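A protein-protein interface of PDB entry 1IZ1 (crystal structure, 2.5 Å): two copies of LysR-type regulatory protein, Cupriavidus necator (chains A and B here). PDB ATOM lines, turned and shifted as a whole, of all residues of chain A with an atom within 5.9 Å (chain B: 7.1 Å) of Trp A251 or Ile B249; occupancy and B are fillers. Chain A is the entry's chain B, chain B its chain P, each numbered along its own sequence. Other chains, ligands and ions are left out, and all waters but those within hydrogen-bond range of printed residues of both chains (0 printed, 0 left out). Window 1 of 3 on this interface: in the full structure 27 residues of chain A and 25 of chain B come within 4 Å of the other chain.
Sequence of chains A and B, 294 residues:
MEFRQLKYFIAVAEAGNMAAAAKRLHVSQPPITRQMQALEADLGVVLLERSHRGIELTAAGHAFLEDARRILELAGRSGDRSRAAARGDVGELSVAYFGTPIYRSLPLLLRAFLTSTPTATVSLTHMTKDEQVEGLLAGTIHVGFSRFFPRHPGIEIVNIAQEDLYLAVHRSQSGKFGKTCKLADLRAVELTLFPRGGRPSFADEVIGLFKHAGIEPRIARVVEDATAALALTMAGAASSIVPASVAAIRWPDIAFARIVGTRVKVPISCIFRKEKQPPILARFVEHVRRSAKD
The side-chain sulfur of Met A234 lies close to the backbone carbonyl oxygen of Tyr B103, 3.6 Å away.
N of Arg A250 sits at hydrogen-bond distance from O of Arg B250 (3.0 Å).
The side-chain carboxylate (OD2) of Asp A253 lies within salt-bridge range of the guanidinium group (NH1) of Arg B104.
The guanidinium group (NH1) of Arg B104 is in hydrogen-bond range of the side-chain sulfur (SD) of Met A234 (3.4 Å).
The backbone carbonyl oxygen (O) of Val B246 is in hydrogen-bond range of the indole nitrogen (NE1) of Trp B251 (3.0 Å).
O of Ile A249 sits close to NE1 of Trp A251 (3.5 Å).
O of Val A246 is in hydrogen-bond range of NE1 of Trp A251 (3.2 Å).
Among the printed residues, pairs that only touch across the chains: Ile A249 with Ile B249 (3.2 Å), Ile A249 with Arg B250 (3.6 Å), Ile A249 with Trp B251 (3.5 Å), Arg A250 with Ile B249 (3.8 Å), Trp A251 with Ile B249 (3.8 Å), Pro A252 with Arg B104 (3.6 Å), Pro A252 with Ala B248 (3.2 Å) and Pro A252 with Ile B249 (3.7 Å).
Of chain B, only Ile B249 comes within 4 Å of Trp A251.
Printed residues of chain A within 4 Å of Ile B249: Ile A249 (3.2 Å), Arg A250 (3.8 Å), Trp A251 (3.8 Å) and Pro A252 (3.7 Å).
Of the printed residues of chain B, Arg A250 touches Ile B249 and Arg B250.
Of the printed residues of chain B, Met A234 touches Tyr B103 and Arg B104.
Of the printed residues of chain B, Asp A253 touches Arg B104.
Of the printed residues of chain A, Arg B104 touches Met A234, Pro A252 and Asp A253.
Of the printed residues of chain B, Pro A252 touches Arg B104 (3.6 Å), Ala B248 (3.2 Å) and Ile B249 (3.7 Å).
Tyr A103 touches none of the printed residues of chain B.
Val A246 touches none of the printed residues of chain B.
The nearest residue of chain A that does not touch Ile B249 is Met A234 (5.1 Å).
Hydrophobic or aromatic side chains of chain A within 4 Å of the printed part of chain B: Met A234, Ile A249, Trp A251 and Pro A252.
Ile B249 touches its own counterpart, Ile A249.
Ile A249 touches Arg B250, and with the chains exchanged Arg A250 touches Ile B249.
Ile A249 touches Trp B251, and with the chains exchanged Trp A251 touches Ile B249.
Arg A250 touches its own counterpart, Arg B250.
Positions printed for both chains: 103, 246, 247, 249, 250, 251, 254 and 256.
Of the 12 pairs that touch across the chains among the printed residues, 6 have their exchanged pair printed and touching as well.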
ATOM      1  N   TYR A 103       4.631  22.732  23.604  1.00  0.00           N
ATOM      2  CA  TYR A 103       3.562  22.297  22.683  1.00  0.00           C
ATOM      3  C   TYR A 103       3.908  22.284  21.209  1.00  0.00           C
ATOM      4  O   TYR A 103       3.287  21.538  20.462  1.00  0.00           O
ATOM      5  CB  TYR A 103       2.291  23.132  22.843  1.00  0.00           C
ATOM      6  CG  TYR A 103       1.579  22.936  24.143  1.00  0.00           C
ATOM      7  CD1 TYR A 103       1.673  23.887  25.139  1.00  0.00           C
ATOM      8  CD2 TYR A 103       0.828  21.800  24.392  1.00  0.00           C
ATOM      9  CE1 TYR A 103       1.049  23.720  26.351  1.00  0.00           C
ATOM     10  CE2 TYR A 103       0.189  21.628  25.620  1.00  0.00           C
ATOM     11  CZ  TYR A 103       0.314  22.607  26.581  1.00  0.00           C
ATOM     12  OH  TYR A 103      -0.294  22.508  27.790  1.00  0.00           O
ATOM     13  N   LEU A 230      -6.818  25.426  29.321  1.00  0.00           N
ATOM     14  CA  LEU A 230      -7.378  24.715  28.177  1.00  0.00           C
ATOM     15  C   LEU A 230      -8.450  23.702  28.578  1.00  0.00           C
ATOM     16  O   LEU A 230      -9.472  23.583  27.929  1.00  0.00           O
ATOM     17  CB  LEU A 230      -6.270  23.997  27.423  1.00  0.00           C
ATOM     18  CG  LEU A 230      -5.329  24.874  26.620  1.00  0.00           C
ATOM     19  CD1 LEU A 230      -4.065  24.137  26.340  1.00  0.00           C
ATOM     20  CD2 LEU A 230      -6.000  25.270  25.324  1.00  0.00           C
ATOM     21  N   MET A 234     -12.231  23.773  27.461  1.00  0.00           N
ATOM     22  CA  MET A 234     -12.855  22.564  26.928  1.00  0.00           C
ATOM     23  C   MET A 234     -14.120  22.211  27.705  1.00  0.00           C
ATOM     24  O   MET A 234     -15.070  21.718  27.141  1.00  0.00           O
ATOM     25  CB  MET A 234     -11.865  21.400  26.960  1.00  0.00           C
ATOM     26  CG  MET A 234     -12.398  20.157  26.268  1.00  0.00           C
ATOM     27  SD  MET A 234     -11.351  18.733  26.448  1.00  0.00           S
ATOM     28  CE  MET A 234      -9.922  19.291  25.613  1.00  0.00           C
ATOM     29  N   VAL A 246      -0.117  26.303  21.027  1.00  0.00           N
ATOM     30  CA  VAL A 246      -1.373  25.774  21.511  1.00  0.00           C
ATOM     31  C   VAL A 246      -2.436  25.794  20.393  1.00  0.00           C
ATOM     32  O   VAL A 246      -3.186  24.811  20.233  1.00  0.00           O
ATOM     33  CB  VAL A 246      -1.827  26.557  22.741  1.00  0.00           C
ATOM     34  CG1 VAL A 246      -3.228  26.141  23.188  1.00  0.00           C
ATOM     35  CG2 VAL A 246      -0.814  26.366  23.860  1.00  0.00           C
ATOM     36  N   ALA A 247      -2.497  26.898  19.629  1.00  0.00           N
ATOM     37  CA  ALA A 247      -3.481  27.024  18.545  1.00  0.00           C
ATOM     38  C   ALA A 247      -3.277  26.001  17.412  1.00  0.00           C
ATOM     39  O   ALA A 247      -4.219  25.620  16.735  1.00  0.00           O
ATOM     40  CB  ALA A 247      -3.496  28.467  17.987  1.00  0.00           C
ATOM     41  N   ILE A 249      -2.485  22.891  17.730  1.00  0.00           N
ATOM     42  CA  ILE A 249      -3.148  21.666  18.112  1.00  0.00           C
ATOM     43  C   ILE A 249      -4.648  21.883  18.030  1.00  0.00           C
ATOM     44  O   ILE A 249      -5.127  22.985  18.253  1.00  0.00           O
ATOM     45  CB  ILE A 249      -2.720  21.291  19.530  1.00  0.00           C
ATOM     46  CG1 ILE A 249      -1.203  21.026  19.544  1.00  0.00           C
ATOM     47  CG2 ILE A 249      -3.519  20.090  20.038  1.00  0.00           C
ATOM     48  CD1 ILE A 249      -0.571  21.148  20.933  1.00  0.00           C
ATOM     49  N   ARG A 250      -5.375  20.817  17.723  1.00  0.00           N
ATOM     50  CA  ARG A 250      -6.812  20.857  17.494  1.00  0.00           C
ATOM     51  C   ARG A 250      -7.522  20.111  18.618  1.00  0.00           C
ATOM     52  O   ARG A 250      -7.585  18.893  18.622  1.00  0.00           O
ATOM     53  CB  ARG A 250      -7.118  20.215  16.136  1.00  0.00           C
ATOM     54  CG  ARG A 250      -8.241  20.854  15.337  1.00  0.00           C
ATOM     55  CD  ARG A 250      -9.533  20.018  15.329  1.00  0.00           C
ATOM     56  NE  ARG A 250     -10.744  20.836  15.191  1.00  0.00           N
ATOM     57  CZ  ARG A 250     -11.995  20.365  15.312  1.00  0.00           C
ATOM     58  NH1 ARG A 250     -12.200  19.071  15.569  1.00  0.00           N
ATOM     59  NH2 ARG A 250     -13.043  21.184  15.162  1.00  0.00           N
ATOM     60  N   TRP A 251      -8.057  20.856  19.583  1.00  0.00           N
ATOM     61  CA  TRP A 251      -8.624  20.247  20.782  1.00  0.00           C
ATOM     62  C   TRP A 251     -10.108  20.065  20.528  1.00  0.00           C
ATOM     63  O   TRP A 251     -10.718  20.879  19.894  1.00  0.00           O
ATOM     64  CB  TRP A 251      -8.385  21.115  22.013  1.00  0.00           C
ATOM     65  CG  TRP A 251      -7.008  21.630  22.097  1.00  0.00           C
ATOM     66  CD1 TRP A 251      -6.471  22.655  21.375  1.00  0.00           C
ATOM     67  CD2 TRP A 251      -5.965  21.165  22.960  1.00  0.00           C
ATOM     68  NE1 TRP A 251      -5.159  22.849  21.726  1.00  0.00           N
ATOM     69  CE2 TRP A 251      -4.825  21.950  22.701  1.00  0.00           C
ATOM     70  CE3 TRP A 251      -5.880  20.164  23.925  1.00  0.00           C
ATOM     71  CZ2 TRP A 251      -3.635  21.755  23.350  1.00  0.00           C
ATOM     72  CZ3 TRP A 251      -4.708  19.973  24.562  1.00  0.00           C
ATOM     73  CH2 TRP A 251      -3.588  20.757  24.276  1.00  0.00           C
ATOM     74  N   PRO A 252     -10.698  18.974  20.944  1.00  0.00           N
ATOM     75  CA  PRO A 252     -12.139  18.863  20.797  1.00  0.00           C
ATOM     76  C   PRO A 252     -12.799  19.911  21.693  1.00  0.00           C
ATOM     77  O   PRO A 252     -12.307  20.176  22.806  1.00  0.00           O
ATOM     78  CB  PRO A 252     -12.430  17.449  21.273  1.00  0.00           C
ATOM     79  CG  PRO A 252     -11.154  16.771  21.180  1.00  0.00           C
ATOM     80  CD  PRO A 252     -10.103  17.768  21.522  1.00  0.00           C
ATOM     81  N   ASP A 253     -13.865  20.518  21.181  1.00  0.00           N
ATOM     82  CA  ASP A 253     -14.623  21.529  21.897  1.00  0.00           C
ATOM     83  C   ASP A 253     -13.910  22.876  22.108  1.00  0.00           C
ATOM     84  O   ASP A 253     -14.478  23.758  22.734  1.00  0.00           O
ATOM     85  CB  ASP A 253     -15.114  20.985  23.263  1.00  0.00           C
ATOM     86  CG  ASP A 253     -15.963  19.748  23.132  1.00  0.00           C
ATOM     87  OD1 ASP A 253     -16.495  19.475  22.055  1.00  0.00           O
ATOM     88  OD2 ASP A 253     -16.165  18.975  24.066  1.00  0.00           O
ATOM     89  N   ILE A 254     -12.689  23.060  21.611  1.00  0.00           N
ATOM     90  CA  ILE A 254     -12.067  24.394  21.703  1.00  0.00           C
ATOM     91  C   ILE A 254     -11.955  24.980  20.303  1.00  0.00           C
ATOM     92  O   ILE A 254     -11.587  24.283  19.372  1.00  0.00           O
ATOM     93  CB  ILE A 254     -10.657  24.376  22.420  1.00  0.00           C
ATOM     94  CG1 ILE A 254     -10.755  23.833  23.852  1.00  0.00           C
ATOM     95  CG2 ILE A 254     -10.037  25.789  22.476  1.00  0.00           C
ATOM     96  CD1 ILE A 254      -9.372  23.615  24.532  1.00  0.00           C
ATOM     97  N   ALA A 255     -12.264  26.271  20.188  1.00  0.00           N
ATOM     98  CA  ALA A 255     -12.150  27.044  18.943  1.00  0.00           C
ATOM     99  C   ALA A 255     -11.205  28.216  19.164  1.00  0.00           C
ATOM    100  O   ALA A 255     -11.209  28.789  20.247  1.00  0.00           O
ATOM    101  CB  ALA A 255     -13.517  27.559  18.514  1.00  0.00           C
ATOM    102  N   PHE A 256     -10.431  28.575  18.124  1.00  0.00           N
ATOM    103  CA  PHE A 256      -9.508  29.706  18.170  1.00  0.00           C
ATOM    104  C   PHE A 256      -9.780  30.787  17.125  1.00  0.00           C
ATOM    105  O   PHE A 256     -10.068  30.477  15.981  1.00  0.00           O
ATOM    106  CB  PHE A 256      -8.076  29.238  17.955  1.00  0.00           C
ATOM    107  CG  PHE A 256      -7.654  28.139  18.864  1.00  0.00           C
ATOM    108  CD1 PHE A 256      -7.774  26.805  18.470  1.00  0.00           C
ATOM    109  CD2 PHE A 256      -7.154  28.420  20.102  1.00  0.00           C
ATOM    110  CE1 PHE A 256      -7.387  25.801  19.304  1.00  0.00           C
ATOM    111  CE2 PHE A 256      -6.760  27.414  20.928  1.00  0.00           C
ATOM    112  CZ  PHE A 256      -6.874  26.111  20.531  1.00  0.00           C
ATOM    113  N   ILE B 102      -6.943  14.715  32.299  1.00  0.00           N
ATOM    114  CA  ILE B 102      -7.067  16.163  32.109  1.00  0.00           C
ATOM    115  C   ILE B 102      -7.204  16.570  30.655  1.00  0.00           C
ATOM    116  O   ILE B 102      -7.596  17.685  30.372  1.00  0.00           O
ATOM    117  CB  ILE B 102      -5.841  16.892  32.729  1.00  0.00           C
ATOM    118  CG1 ILE B 102      -6.045  18.403  32.798  1.00  0.00           C
ATOM    119  CG2 ILE B 102      -4.579  16.647  31.931  1.00  0.00           C
ATOM    120  CD1 ILE B 102      -7.283  18.841  33.486  1.00  0.00           C
ATOM    121  N   TYR B 103      -6.847  15.680  29.733  1.00  0.00           N
ATOM    122  CA  TYR B 103      -6.816  16.013  28.311  1.00  0.00           C
ATOM    123  C   TYR B 103      -8.207  16.023  27.680  1.00  0.00           C
ATOM    124  O   TYR B 103      -8.422  16.743  26.712  1.00  0.00           O
ATOM    125  CB  TYR B 103      -5.895  15.053  27.543  1.00  0.00           C
ATOM    126  CG  TYR B 103      -4.424  15.354  27.737  1.00  0.00           C
ATOM    127  CD1 TYR B 103      -3.790  15.074  28.939  1.00  0.00           C
ATOM    128  CD2 TYR B 103      -3.673  15.930  26.734  1.00  0.00           C
ATOM    129  CE1 TYR B 103      -2.435  15.352  29.129  1.00  0.00           C
ATOM    130  CE2 TYR B 103      -2.338  16.214  26.920  1.00  0.00           C
ATOM    131  CZ  TYR B 103      -1.728  15.918  28.122  1.00  0.00           C
ATOM    132  OH  TYR B 103      -0.404  16.192  28.293  1.00  0.00           O
ATOM    133  N   ARG B 104      -9.130  15.227  28.227  1.00  0.00           N
ATOM    134  CA  ARG B 104     -10.446  15.019  27.627  1.00  0.00           C
ATOM    135  C   ARG B 104     -11.512  14.475  28.598  1.00  0.00           C
ATOM    136  O   ARG B 104     -12.533  15.123  28.821  1.00  0.00           O
ATOM    137  CB  ARG B 104     -10.340  14.078  26.436  1.00  0.00           C
ATOM    138  CG  ARG B 104     -11.669  13.903  25.632  1.00  0.00           C
ATOM    139  CD  ARG B 104     -12.171  15.235  25.053  1.00  0.00           C
ATOM    140  NE  ARG B 104     -13.408  15.197  24.280  1.00  0.00           N
ATOM    141  CZ  ARG B 104     -14.255  16.229  24.175  1.00  0.00           C
ATOM    142  NH1 ARG B 104     -14.030  17.381  24.812  1.00  0.00           N
ATOM    143  NH2 ARG B 104     -15.343  16.117  23.441  1.00  0.00           N
ATOM    144  N   ALA B 244      -7.113   7.310  25.511  1.00  0.00           N
ATOM    145  CA  ALA B 244      -7.930   7.878  24.450  1.00  0.00           C
ATOM    146  C   ALA B 244      -8.079   9.394  24.574  1.00  0.00           C
ATOM    147  O   ALA B 244      -8.257  10.074  23.563  1.00  0.00           O
ATOM    148  CB  ALA B 244      -9.330   7.195  24.422  1.00  0.00           C
ATOM    149  N   SER B 245      -7.995   9.911  25.794  1.00  0.00           N
ATOM    150  CA  SER B 245      -8.065  11.346  26.030  1.00  0.00           C
ATOM    151  C   SER B 245      -6.988  12.126  25.254  1.00  0.00           C
ATOM    152  O   SER B 245      -7.226  13.247  24.775  1.00  0.00           O
ATOM    153  CB  SER B 245      -7.941  11.640  27.525  1.00  0.00           C
ATOM    154  OG  SER B 245      -9.148  11.327  28.237  1.00  0.00           O
ATOM    155  N   VAL B 246      -5.804  11.545  25.131  1.00  0.00           N
ATOM    156  CA  VAL B 246      -4.702  12.198  24.427  1.00  0.00           C
ATOM    157  C   VAL B 246      -4.892  12.029  22.941  1.00  0.00           C
ATOM    158  O   VAL B 246      -4.619  12.945  22.186  1.00  0.00           O
ATOM    159  CB  VAL B 246      -3.334  11.604  24.823  1.00  0.00           C
ATOM    160  CG1 VAL B 246      -2.240  12.183  23.980  1.00  0.00           C
ATOM    161  CG2 VAL B 246      -3.035  11.813  26.296  1.00  0.00           C
ATOM    162  N   ALA B 247      -5.360  10.850  22.521  1.00  0.00           N
ATOM    163  CA  ALA B 247      -5.566  10.549  21.098  1.00  0.00           C
ATOM    164  C   ALA B 247      -6.791  11.250  20.475  1.00  0.00           C
ATOM    165  O   ALA B 247      -6.885  11.377  19.260  1.00  0.00           O
ATOM    166  CB  ALA B 247      -5.661   9.032  20.902  1.00  0.00           C
ATOM    167  N   ALA B 248      -7.717  11.721  21.306  1.00  0.00           N
ATOM    168  CA  ALA B 248      -8.864  12.498  20.846  1.00  0.00           C
ATOM    169  C   ALA B 248      -8.465  13.895  20.363  1.00  0.00           C
ATOM    170  O   ALA B 248      -9.287  14.594  19.796  1.00  0.00           O
ATOM    171  CB  ALA B 248      -9.818  12.642  21.960  1.00  0.00           C
ATOM    172  N   ILE B 249      -7.222  14.299  20.653  1.00  0.00           N
ATOM    173  CA  ILE B 249      -6.649  15.570  20.244  1.00  0.00           C
ATOM    174  C   ILE B 249      -5.765  15.349  19.019  1.00  0.00           C
ATOM    175  O   ILE B 249      -5.156  14.276  18.844  1.00  0.00           O
ATOM    176  CB  ILE B 249      -5.829  16.187  21.422  1.00  0.00           C
ATOM    177  CG1 ILE B 249      -6.761  16.593  22.562  1.00  0.00           C
ATOM    178  CG2 ILE B 249      -5.033  17.412  21.003  1.00  0.00           C
ATOM    179  CD1 ILE B 249      -6.143  16.413  23.896  1.00  0.00           C
ATOM    180  N   ARG B 250      -5.697  16.367  18.170  1.00  0.00           N
ATOM    181  CA  ARG B 250      -4.988  16.283  16.914  1.00  0.00           C
ATOM    182  C   ARG B 250      -3.727  17.132  17.006  1.00  0.00           C
ATOM    183  O   ARG B 250      -3.780  18.362  16.915  1.00  0.00           O
ATOM    184  CB  ARG B 250      -5.896  16.741  15.779  1.00  0.00           C
ATOM    185  CG  ARG B 250      -5.807  15.882  14.542  1.00  0.00           C
ATOM    186  CD  ARG B 250      -6.628  16.422  13.341  1.00  0.00           C
ATOM    187  NE  ARG B 250      -5.888  16.345  12.064  1.00  0.00           N
ATOM    188  CZ  ARG B 250      -6.274  16.919  10.917  1.00  0.00           C
ATOM    189  NH1 ARG B 250      -7.391  17.651  10.852  1.00  0.00           N
ATOM    190  NH2 ARG B 250      -5.530  16.760   9.825  1.00  0.00           N
ATOM    191  N   TRP B 251      -2.602  16.461  17.205  1.00  0.00           N
ATOM    192  CA  TRP B 251      -1.308  17.096  17.411  1.00  0.00           C
ATOM    193  C   TRP B 251      -0.565  17.046  16.087  1.00  0.00           C
ATOM    194  O   TRP B 251      -0.514  16.009  15.438  1.00  0.00           O
ATOM    195  CB  TRP B 251      -0.480  16.339  18.463  1.00  0.00           C
ATOM    196  CG  TRP B 251      -1.211  15.982  19.715  1.00  0.00           C
ATOM    197  CD1 TRP B 251      -2.100  14.966  19.886  1.00  0.00           C
ATOM    198  CD2 TRP B 251      -1.104  16.635  20.966  1.00  0.00           C
ATOM    199  NE1 TRP B 251      -2.572  14.956  21.177  1.00  0.00           N
ATOM    200  CE2 TRP B 251      -1.967  15.974  21.865  1.00  0.00           C
ATOM    201  CE3 TRP B 251      -0.357  17.707  21.431  1.00  0.00           C
ATOM    202  CZ2 TRP B 251      -2.109  16.364  23.186  1.00  0.00           C
ATOM    203  CZ3 TRP B 251      -0.497  18.090  22.737  1.00  0.00           C
ATOM    204  CH2 TRP B 251      -1.372  17.428  23.597  1.00  0.00           C
ATOM    205  N   ILE B 254       1.986  14.005  14.941  1.00  0.00           N
ATOM    206  CA  ILE B 254       1.758  12.776  15.686  1.00  0.00           C
ATOM    207  C   ILE B 254       0.567  12.062  15.076  1.00  0.00           C
ATOM    208  O   ILE B 254      -0.428  12.688  14.716  1.00  0.00           O
ATOM    209  CB  ILE B 254       1.520  13.014  17.181  1.00  0.00           C
ATOM    210  CG1 ILE B 254       2.520  14.024  17.771  1.00  0.00           C
ATOM    211  CG2 ILE B 254       1.651  11.709  17.933  1.00  0.00           C
ATOM    212  CD1 ILE B 254       2.527  14.048  19.314  1.00  0.00           C
ATOM    213  N   PHE B 256      -1.889   8.318  15.450  1.00  0.00           N
ATOM    214  CA  PHE B 256      -2.431   7.406  16.444  1.00  0.00           C
ATOM    215  C   PHE B 256      -3.122   6.171  15.818  1.00  0.00           C
ATOM    216  O   PHE B 256      -3.934   6.296  14.913  1.00  0.00           O
ATOM    217  CB  PHE B 256      -3.477   8.124  17.330  1.00  0.00           C
ATOM    218  CG  PHE B 256      -2.943   9.264  18.139  1.00  0.00           C
ATOM    219  CD1 PHE B 256      -3.311  10.562  17.848  1.00  0.00           C
ATOM    220  CD2 PHE B 256      -2.105   9.037  19.217  1.00  0.00           C
ATOM    221  CE1 PHE B 256      -2.815  11.633  18.607  1.00  0.00           C
ATOM    222  CE2 PHE B 256      -1.621  10.092  19.986  1.00  0.00           C
ATOM    223  CZ  PHE B 256      -1.979  11.396  19.678  1.00  0.00           C
